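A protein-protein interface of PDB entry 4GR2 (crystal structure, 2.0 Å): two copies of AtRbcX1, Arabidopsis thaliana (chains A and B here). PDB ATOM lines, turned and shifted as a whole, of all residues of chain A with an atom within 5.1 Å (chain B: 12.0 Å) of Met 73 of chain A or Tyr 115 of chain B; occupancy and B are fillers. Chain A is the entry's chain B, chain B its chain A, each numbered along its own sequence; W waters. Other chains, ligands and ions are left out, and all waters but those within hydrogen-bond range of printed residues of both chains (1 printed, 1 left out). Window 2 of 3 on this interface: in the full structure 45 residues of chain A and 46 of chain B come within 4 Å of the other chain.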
ATOM      1  N   LEU A  65      13.097  -4.161   8.335  1.00  0.00           N
ATOM      2  CA  LEU A  65      11.771  -3.571   8.205  1.00  0.00           C
ATOM      3  C   LEU A  65      11.207  -3.723   6.794  1.00  0.00           C
ATOM      4  O   LEU A  65      10.011  -3.914   6.602  1.00  0.00           O
ATOM      5  CB  LEU A  65      11.808  -2.094   8.576  1.00  0.00           C
ATOM      6  CG  LEU A  65      10.463  -1.369   8.520  1.00  0.00           C
ATOM      7  CD1 LEU A  65       9.484  -1.936   9.555  1.00  0.00           C
ATOM      8  CD2 LEU A  65      10.660   0.151   8.681  1.00  0.00           C
ATOM      9  N   MET A  66      12.044  -3.629   5.782  1.00  0.00           N
ATOM     10  CA  MET A  66      11.446  -3.684   4.458  1.00  0.00           C
ATOM     11  C   MET A  66      11.250  -5.100   3.933  1.00  0.00           C
ATOM     12  O   MET A  66      10.611  -5.307   2.899  1.00  0.00           O
ATOM     13  CB  MET A  66      12.181  -2.808   3.469  1.00  0.00           C
ATOM     14  CG  MET A  66      13.610  -3.096   3.335  1.00  0.00           C
ATOM     15  SD  MET A  66      14.392  -1.525   2.960  1.00  0.00           S
ATOM     16  CE  MET A  66      15.753  -2.088   1.975  1.00  0.00           C
ATOM     17  N   ARG A  67      11.786  -6.066   4.662  1.00  0.00           N
ATOM     18  CA  ARG A  67      11.586  -7.467   4.339  1.00  0.00           C
ATOM     19  C   ARG A  67      10.423  -8.016   5.160  1.00  0.00           C
ATOM     20  O   ARG A  67       9.998  -9.150   4.961  1.00  0.00           O
ATOM     21  CB  ARG A  67      12.864  -8.257   4.602  1.00  0.00           C
ATOM     22  CG  ARG A  67      13.890  -8.114   3.499  1.00  0.00           C
ATOM     23  CD  ARG A  67      15.277  -8.509   3.964  1.00  0.00           C
ATOM     24  NE  ARG A  67      16.275  -8.345   2.906  1.00  0.00           N
ATOM     25  CZ  ARG A  67      16.725  -7.171   2.456  1.00  0.00           C
ATOM     26  NH1 ARG A  67      16.273  -6.023   2.957  1.00  0.00           N
ATOM     27  NH2 ARG A  67      17.641  -7.143   1.501  1.00  0.00           N
ATOM     28  N   SER A  69       7.163  -6.908   5.319  1.00  0.00           N
ATOM     29  CA  SER A  69       5.991  -7.044   4.467  1.00  0.00           C
ATOM     30  C   SER A  69       6.091  -5.959   3.411  1.00  0.00           C
ATOM     31  O   SER A  69       6.948  -5.084   3.507  1.00  0.00           O
ATOM     32  CB  SER A  69       4.688  -6.929   5.276  1.00  0.00           C
ATOM     33  OG  SER A  69       4.214  -5.600   5.390  1.00  0.00           O
ATOM     34  N   SER A  70       5.237  -6.026   2.394  1.00  0.00           N
ATOM     35  CA  SER A  70       5.229  -5.005   1.366  1.00  0.00           C
ATOM     36  C   SER A  70       4.888  -3.628   1.963  1.00  0.00           C
ATOM     37  O   SER A  70       5.508  -2.612   1.611  1.00  0.00           O
ATOM     38  CB  SER A  70       4.244  -5.389   0.246  1.00  0.00           C
ATOM     39  OG  SER A  70       2.958  -5.661   0.789  1.00  0.00           O
ATOM     40  N   ARG A  71       3.931  -3.580   2.889  1.00  0.00           N
ATOM     41  CA  ARG A  71       3.589  -2.289   3.488  1.00  0.00           C
ATOM     42  C   ARG A  71       4.654  -1.791   4.486  1.00  0.00           C
ATOM     43  O   ARG A  71       4.867  -0.593   4.631  1.00  0.00           O
ATOM     44  CB  ARG A  71       2.188  -2.308   4.102  1.00  0.00           C
ATOM     45  CG  ARG A  71       2.094  -2.940   5.448  1.00  0.00           C
ATOM     46  CD  ARG A  71       0.696  -3.551   5.658  1.00  0.00           C
ATOM     47  NE  ARG A  71       0.674  -4.357   6.882  1.00  0.00           N
ATOM     48  CZ  ARG A  71       0.978  -5.650   6.931  1.00  0.00           C
ATOM     49  NH1 ARG A  71       1.297  -6.297   5.821  1.00  0.00           N
ATOM     50  NH2 ARG A  71       0.951  -6.297   8.091  1.00  0.00           N
ATOM     51  N   HIS A  72       5.340  -2.712   5.151  1.00  0.00           N
ATOM     52  CA  HIS A  72       6.471  -2.327   5.979  1.00  0.00           C
ATOM     53  C   HIS A  72       7.582  -1.783   5.079  1.00  0.00           C
ATOM     54  O   HIS A  72       8.297  -0.850   5.447  1.00  0.00           O
ATOM     55  CB  HIS A  72       6.977  -3.528   6.773  1.00  0.00           C
ATOM     56  CG  HIS A  72       6.076  -3.926   7.902  1.00  0.00           C
ATOM     57  ND1 HIS A  72       5.045  -4.831   7.753  1.00  0.00           N
ATOM     58  CD2 HIS A  72       6.050  -3.539   9.199  1.00  0.00           C
ATOM     59  CE1 HIS A  72       4.420  -4.978   8.908  1.00  0.00           C
ATOM     60  NE2 HIS A  72       5.016  -4.211   9.804  1.00  0.00           N
ATOM     61  N   MET A  73       7.707  -2.366   3.889  1.00  0.00           N
ATOM     62  CA  MET A  73       8.699  -1.925   2.918  1.00  0.00           C
ATOM     63  C   MET A  73       8.419  -0.487   2.522  1.00  0.00           C
ATOM     64  O   MET A  73       9.336   0.329   2.407  1.00  0.00           O
ATOM     65  CB  MET A  73       8.722  -2.835   1.698  1.00  0.00           C
ATOM     66  CG  MET A  73       9.885  -2.565   0.759  1.00  0.00           C
ATOM     67  SD  MET A  73       9.428  -1.321  -0.435  1.00  0.00           S
ATOM     68  CE  MET A  73      10.784  -1.442  -1.600  1.00  0.00           C
ATOM     69  N   ASN A  74       7.143  -0.172   2.348  1.00  0.00           N
ATOM     70  CA  ASN A  74       6.762   1.207   2.069  1.00  0.00           C
ATOM     71  C   ASN A  74       7.054   2.136   3.254  1.00  0.00           C
ATOM     72  O   ASN A  74       7.333   3.328   3.068  1.00  0.00           O
ATOM     73  CB  ASN A  74       5.290   1.299   1.642  1.00  0.00           C
ATOM     74  CG  ASN A  74       5.025   0.691   0.240  1.00  0.00           C
ATOM     75  OD1 ASN A  74       5.813   0.863  -0.700  1.00  0.00           O
ATOM     76  ND2 ASN A  74       3.907  -0.019   0.113  1.00  0.00           N
ATOM     77  N   LEU A  75       7.004   1.597   4.471  1.00  0.00           N
ATOM     78  CA  LEU A  75       7.349   2.394   5.648  1.00  0.00           C
ATOM     79  C   LEU A  75       8.859   2.682   5.707  1.00  0.00           C
ATOM     80  O   LEU A  75       9.288   3.800   6.007  1.00  0.00           O
ATOM     81  CB  LEU A  75       6.889   1.685   6.912  1.00  0.00           C
ATOM     82  CG  LEU A  75       6.742   2.567   8.147  1.00  0.00           C
ATOM     83  CD1 LEU A  75       5.918   3.789   7.795  1.00  0.00           C
ATOM     84  CD2 LEU A  75       6.078   1.785   9.271  1.00  0.00           C
ATOM     85  N   ALA A  76       9.655   1.662   5.413  1.00  0.00           N
ATOM     86  CA  ALA A  76      11.094   1.819   5.281  1.00  0.00           C
ATOM     87  C   ALA A  76      11.477   2.904   4.280  1.00  0.00           C
ATOM     88  O   ALA A  76      12.371   3.713   4.550  1.00  0.00           O
ATOM     89  CB  ALA A  76      11.722   0.510   4.871  1.00  0.00           C
ATOM     90  N   LEU A  77      10.818   2.893   3.115  1.00  0.00           N
ATOM     91  CA  LEU A  77      11.114   3.841   2.036  1.00  0.00           C
ATOM     92  C   LEU A  77      10.749   5.268   2.437  1.00  0.00           C
ATOM     93  O   LEU A  77      11.368   6.237   1.978  1.00  0.00           O
ATOM     94  CB  LEU A  77      10.379   3.431   0.743  1.00  0.00           C
ATOM     95  CG  LEU A  77      11.236   2.711  -0.312  1.00  0.00           C
ATOM     96  CD1 LEU A  77      12.271   3.674  -0.895  1.00  0.00           C
ATOM     97  CD2 LEU A  77      11.952   1.498   0.241  1.00  0.00           C
ATOM     98  N   ASP B 106      24.726   6.726   0.219  1.00  0.00           N
ATOM     99  CA  ASP B 106      25.199   5.379  -0.086  1.00  0.00           C
ATOM    100  C   ASP B 106      24.321   4.316   0.576  1.00  0.00           C
ATOM    101  O   ASP B 106      24.075   3.258  -0.011  1.00  0.00           O
ATOM    102  CB  ASP B 106      26.647   5.174   0.345  1.00  0.00           C
ATOM    103  CG  ASP B 106      27.633   5.966  -0.487  1.00  0.00           C
ATOM    104  OD1 ASP B 106      27.242   6.545  -1.530  1.00  0.00           O
ATOM    105  OD2 ASP B 106      28.819   6.005  -0.088  1.00  0.00           O
ATOM    106  N   SER B 107      23.848   4.600   1.786  1.00  0.00           N
ATOM    107  CA  SER B 107      22.978   3.668   2.501  1.00  0.00           C
ATOM    108  C   SER B 107      21.651   3.477   1.775  1.00  0.00           C
ATOM    109  O   SER B 107      21.154   2.350   1.672  1.00  0.00           O
ATOM    110  CB  SER B 107      22.718   4.142   3.930  1.00  0.00           C
ATOM    111  OG  SER B 107      21.580   3.504   4.513  1.00  0.00           O
ATOM    112  N   ASN B 108      21.061   4.581   1.323  1.00  0.00           N
ATOM    113  CA  ASN B 108      19.804   4.523   0.582  1.00  0.00           C
ATOM    114  C   ASN B 108      19.948   3.608  -0.632  1.00  0.00           C
ATOM    115  O   ASN B 108      19.150   2.697  -0.843  1.00  0.00           O
ATOM    116  CB  ASN B 108      19.390   5.914   0.106  1.00  0.00           C
ATOM    117  CG  ASN B 108      18.801   6.769   1.215  1.00  0.00           C
ATOM    118  OD1 ASN B 108      18.454   6.273   2.292  1.00  0.00           O
ATOM    119  ND2 ASN B 108      18.677   8.066   0.951  1.00  0.00           N
ATOM    120  N   THR B 109      20.999   3.860  -1.409  1.00  0.00           N
ATOM    121  CA  THR B 109      21.280   3.127  -2.635  1.00  0.00           C
ATOM    122  C   THR B 109      21.489   1.633  -2.390  1.00  0.00           C
ATOM    123  O   THR B 109      20.944   0.793  -3.111  1.00  0.00           O
ATOM    124  CB  THR B 109      22.501   3.732  -3.366  1.00  0.00           C
ATOM    125  OG1 THR B 109      22.169   5.049  -3.818  1.00  0.00           O
ATOM    126  CG2 THR B 109      22.911   2.886  -4.566  1.00  0.00           C
ATOM    127  N   ARG B 110      22.267   1.307  -1.363  1.00  0.00           N
ATOM    128  CA  ARG B 110      22.581  -0.073  -1.043  1.00  0.00           C
ATOM    129  C   ARG B 110      21.356  -0.805  -0.492  1.00  0.00           C
ATOM    130  O   ARG B 110      21.090  -1.939  -0.886  1.00  0.00           O
ATOM    131  CB  ARG B 110      23.746  -0.130  -0.048  1.00  0.00           C
ATOM    132  CG  ARG B 110      24.336  -1.509   0.178  1.00  0.00           C
ATOM    133  CD  ARG B 110      25.497  -1.461   1.177  1.00  0.00           C
ATOM    134  NE  ARG B 110      25.336  -0.378   2.152  1.00  0.00           N
ATOM    135  CZ  ARG B 110      26.117   0.701   2.226  1.00  0.00           C
ATOM    136  NH1 ARG B 110      27.139   0.855   1.394  1.00  0.00           N
ATOM    137  NH2 ARG B 110      25.878   1.630   3.141  1.00  0.00           N
ATOM    138  N   LEU B 111      20.604  -0.167   0.405  1.00  0.00           N
ATOM    139  CA  LEU B 111      19.373  -0.788   0.916  1.00  0.00           C
ATOM    140  C   LEU B 111      18.426  -1.136  -0.237  1.00  0.00           C
ATOM    141  O   LEU B 111      17.787  -2.190  -0.242  1.00  0.00           O
ATOM    142  CB  LEU B 111      18.663   0.115   1.951  1.00  0.00           C
ATOM    143  CG  LEU B 111      19.365   0.272   3.329  1.00  0.00           C
ATOM    144  CD1 LEU B 111      18.720   1.334   4.180  1.00  0.00           C
ATOM    145  CD2 LEU B 111      19.358  -1.029   4.091  1.00  0.00           C
ATOM    146  N   MET B 112      18.351  -0.248  -1.224  1.00  0.00           N
ATOM    147  CA  MET B 112      17.447  -0.441  -2.361  1.00  0.00           C
ATOM    148  C   MET B 112      17.912  -1.566  -3.266  1.00  0.00           C
ATOM    149  O   MET B 112      17.161  -2.504  -3.540  1.00  0.00           O
ATOM    150  CB  MET B 112      17.301   0.859  -3.163  1.00  0.00           C
ATOM    151  CG  MET B 112      16.418   1.875  -2.476  1.00  0.00           C
ATOM    152  SD  MET B 112      15.005   1.068  -1.686  1.00  0.00           S
ATOM    153  CE  MET B 112      14.057   0.515  -3.128  1.00  0.00           C
ATOM    154  N   ARG B 113      19.155  -1.456  -3.730  1.00  0.00           N
ATOM    155  CA  ARG B 113      19.756  -2.465  -4.588  1.00  0.00           C
ATOM    156  C   ARG B 113      19.624  -3.854  -3.984  1.00  0.00           C
ATOM    157  O   ARG B 113      19.138  -4.773  -4.649  1.00  0.00           O
ATOM    158  CB  ARG B 113      21.220  -2.140  -4.884  1.00  0.00           C
ATOM    159  CG  ARG B 113      21.391  -0.919  -5.763  1.00  0.00           C
ATOM    160  CD  ARG B 113      22.829  -0.752  -6.212  1.00  0.00           C
ATOM    161  NE  ARG B 113      23.270  -1.842  -7.085  1.00  0.00           N
ATOM    162  CZ  ARG B 113      23.308  -1.772  -8.414  1.00  0.00           C
ATOM    163  NH1 ARG B 113      22.928  -0.661  -9.043  1.00  0.00           N
ATOM    164  NH2 ARG B 113      23.734  -2.814  -9.114  1.00  0.00           N
ATOM    165  N   GLU B 114      20.008  -3.998  -2.719  1.00  0.00           N
ATOM    166  CA  GLU B 114      20.016  -5.315  -2.080  1.00  0.00           C
ATOM    167  C   GLU B 114      18.630  -5.923  -1.837  1.00  0.00           C
ATOM    168  O   GLU B 114      18.469  -7.147  -1.875  1.00  0.00           O
ATOM    169  CB  GLU B 114      20.835  -5.283  -0.796  1.00  0.00           C
ATOM    170  CG  GLU B 114      22.278  -4.894  -1.060  1.00  0.00           C
ATOM    171  CD  GLU B 114      23.136  -4.869   0.191  1.00  0.00           C
ATOM    172  OE1 GLU B 114      22.581  -4.930   1.312  1.00  0.00           O
ATOM    173  OE2 GLU B 114      24.374  -4.789   0.038  1.00  0.00           O
ATOM    174  N   TYR B 115      17.627  -5.084  -1.603  1.00  0.00           N
ATOM    175  CA  TYR B 115      16.266  -5.595  -1.445  1.00  0.00           C
ATOM    176  C   TYR B 115      15.660  -6.181  -2.740  1.00  0.00           C
ATOM    177  O   TYR B 115      14.969  -7.200  -2.691  1.00  0.00           O
ATOM    178  CB  TYR B 115      15.335  -4.522  -0.884  1.00  0.00           C
ATOM    179  CG  TYR B 115      13.884  -4.965  -0.812  1.00  0.00           C
ATOM    180  CD1 TYR B 115      13.431  -5.720   0.262  1.00  0.00           C
ATOM    181  CD2 TYR B 115      12.970  -4.633  -1.822  1.00  0.00           C
ATOM    182  CE1 TYR B 115      12.110  -6.132   0.352  1.00  0.00           C
ATOM    183  CE2 TYR B 115      11.628  -5.041  -1.746  1.00  0.00           C
ATOM    184  CZ  TYR B 115      11.209  -5.798  -0.647  1.00  0.00           C
ATOM    185  OH  TYR B 115       9.902  -6.231  -0.520  1.00  0.00           O
ATOM    186  N   VAL B 116      15.902  -5.540  -3.884  1.00  0.00           N
ATOM    187  CA  VAL B 116      15.335  -6.022  -5.149  1.00  0.00           C
ATOM    188  C   VAL B 116      16.282  -6.966  -5.902  1.00  0.00           C
ATOM    189  O   VAL B 116      15.880  -7.611  -6.875  1.00  0.00           O
ATOM    190  CB  VAL B 116      14.886  -4.872  -6.099  1.00  0.00           C
ATOM    191  CG1 VAL B 116      14.389  -3.666  -5.316  1.00  0.00           C
ATOM    192  CG2 VAL B 116      16.007  -4.485  -7.020  1.00  0.00           C
ATOM    193  N   LEU B 117      17.532  -7.048  -5.455  1.00  0.00           N
ATOM    194  CA  LEU B 117      18.481  -7.981  -6.043  1.00  0.00           C
ATOM    195  C   LEU B 117      18.675  -9.171  -5.103  1.00  0.00           C
ATOM    196  O   LEU B 117      19.071 -10.258  -5.529  1.00  0.00           O
ATOM    197  CB  LEU B 117      19.817  -7.290  -6.320  1.00  0.00           C
HETATM  198  O   HOH W   1      18.242  -4.233   1.896  1.00  0.00           O
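Of the 12 printed residues of chain A, 4 touch a printed residue of chain B.
Printed residues of chain B that touch a printed residue of chain A: Leu 111, Met 112, Glu 114 and Tyr 115.
Hydrophobic or aromatic side chains of chain B within 4 Å of the printed part of chain A: Leu 111, Met 112 and Tyr 115.
Along chain B the printed residues that touch a printed residue of chain A span positions 111 to 115.
Water W1 bridges NH1 of Arg 67 of chain A (2.9 Å) and O of Leu 111 of chain B (3.0 Å).
Among the printed residues, merely in contact across the chains: Met 66 of chain A with Leu 111 of chain B (3.0 Å), Met 66 of chain A with Tyr 115 of chain B (3.1 Å), Arg 67 of chain A with Tyr 115 of chain B (3.6 Å), Leu 77 of chain A with Met 112 of chain B (3.6 Å) and Met 73 of chain A with Tyr 115 of chain B (3.7 Å).
No residue of chain B comes within 4 Å of Leu 65 of chain A.
Of chain B, only Glu 114 (3.5 Å) and Tyr 115 (3.6 Å) come within 4 Å of Arg 67 of chain A.
No residue of chain B comes within 4 Å of Ser 69 of chain A.
No residue of chain B comes within 4 Å of Ser 70 of chain A.
No residue of chain B comes within 4 Å of His 72 of chain A.
Met 73 of chain A touches just one residue of chain B: Tyr 115 (3.7 Å).
Of the printed residues of chain A, Leu 111 of chain B touches Met 66.
Printed residues of chain A within 4 Å of Met 112 of chain B: Leu 77 (3.6 Å).
Of the printed residues of chain A, Glu 114 of chain B touches Arg 67.
Of the printed residues of chain A, Tyr 115 of chain B touches Met 66 (3.1 Å), Arg 67 (3.6 Å) and Met 73 (3.7 Å).
Leu 117 of chain B touches none of the printed residues of chain A.
The nearest residue of chain B that does not touch Met 73 of chain A is Met 112 of chain B (4.1 Å).
No position is printed for both chains.
Of the 6 pairs that touch across the chains among the printed residues, none has its exchanged pair printed and touching as well.
O of Glu 114 of chain B is in hydrogen-bond range of NH2 of Arg 67 of chain A.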
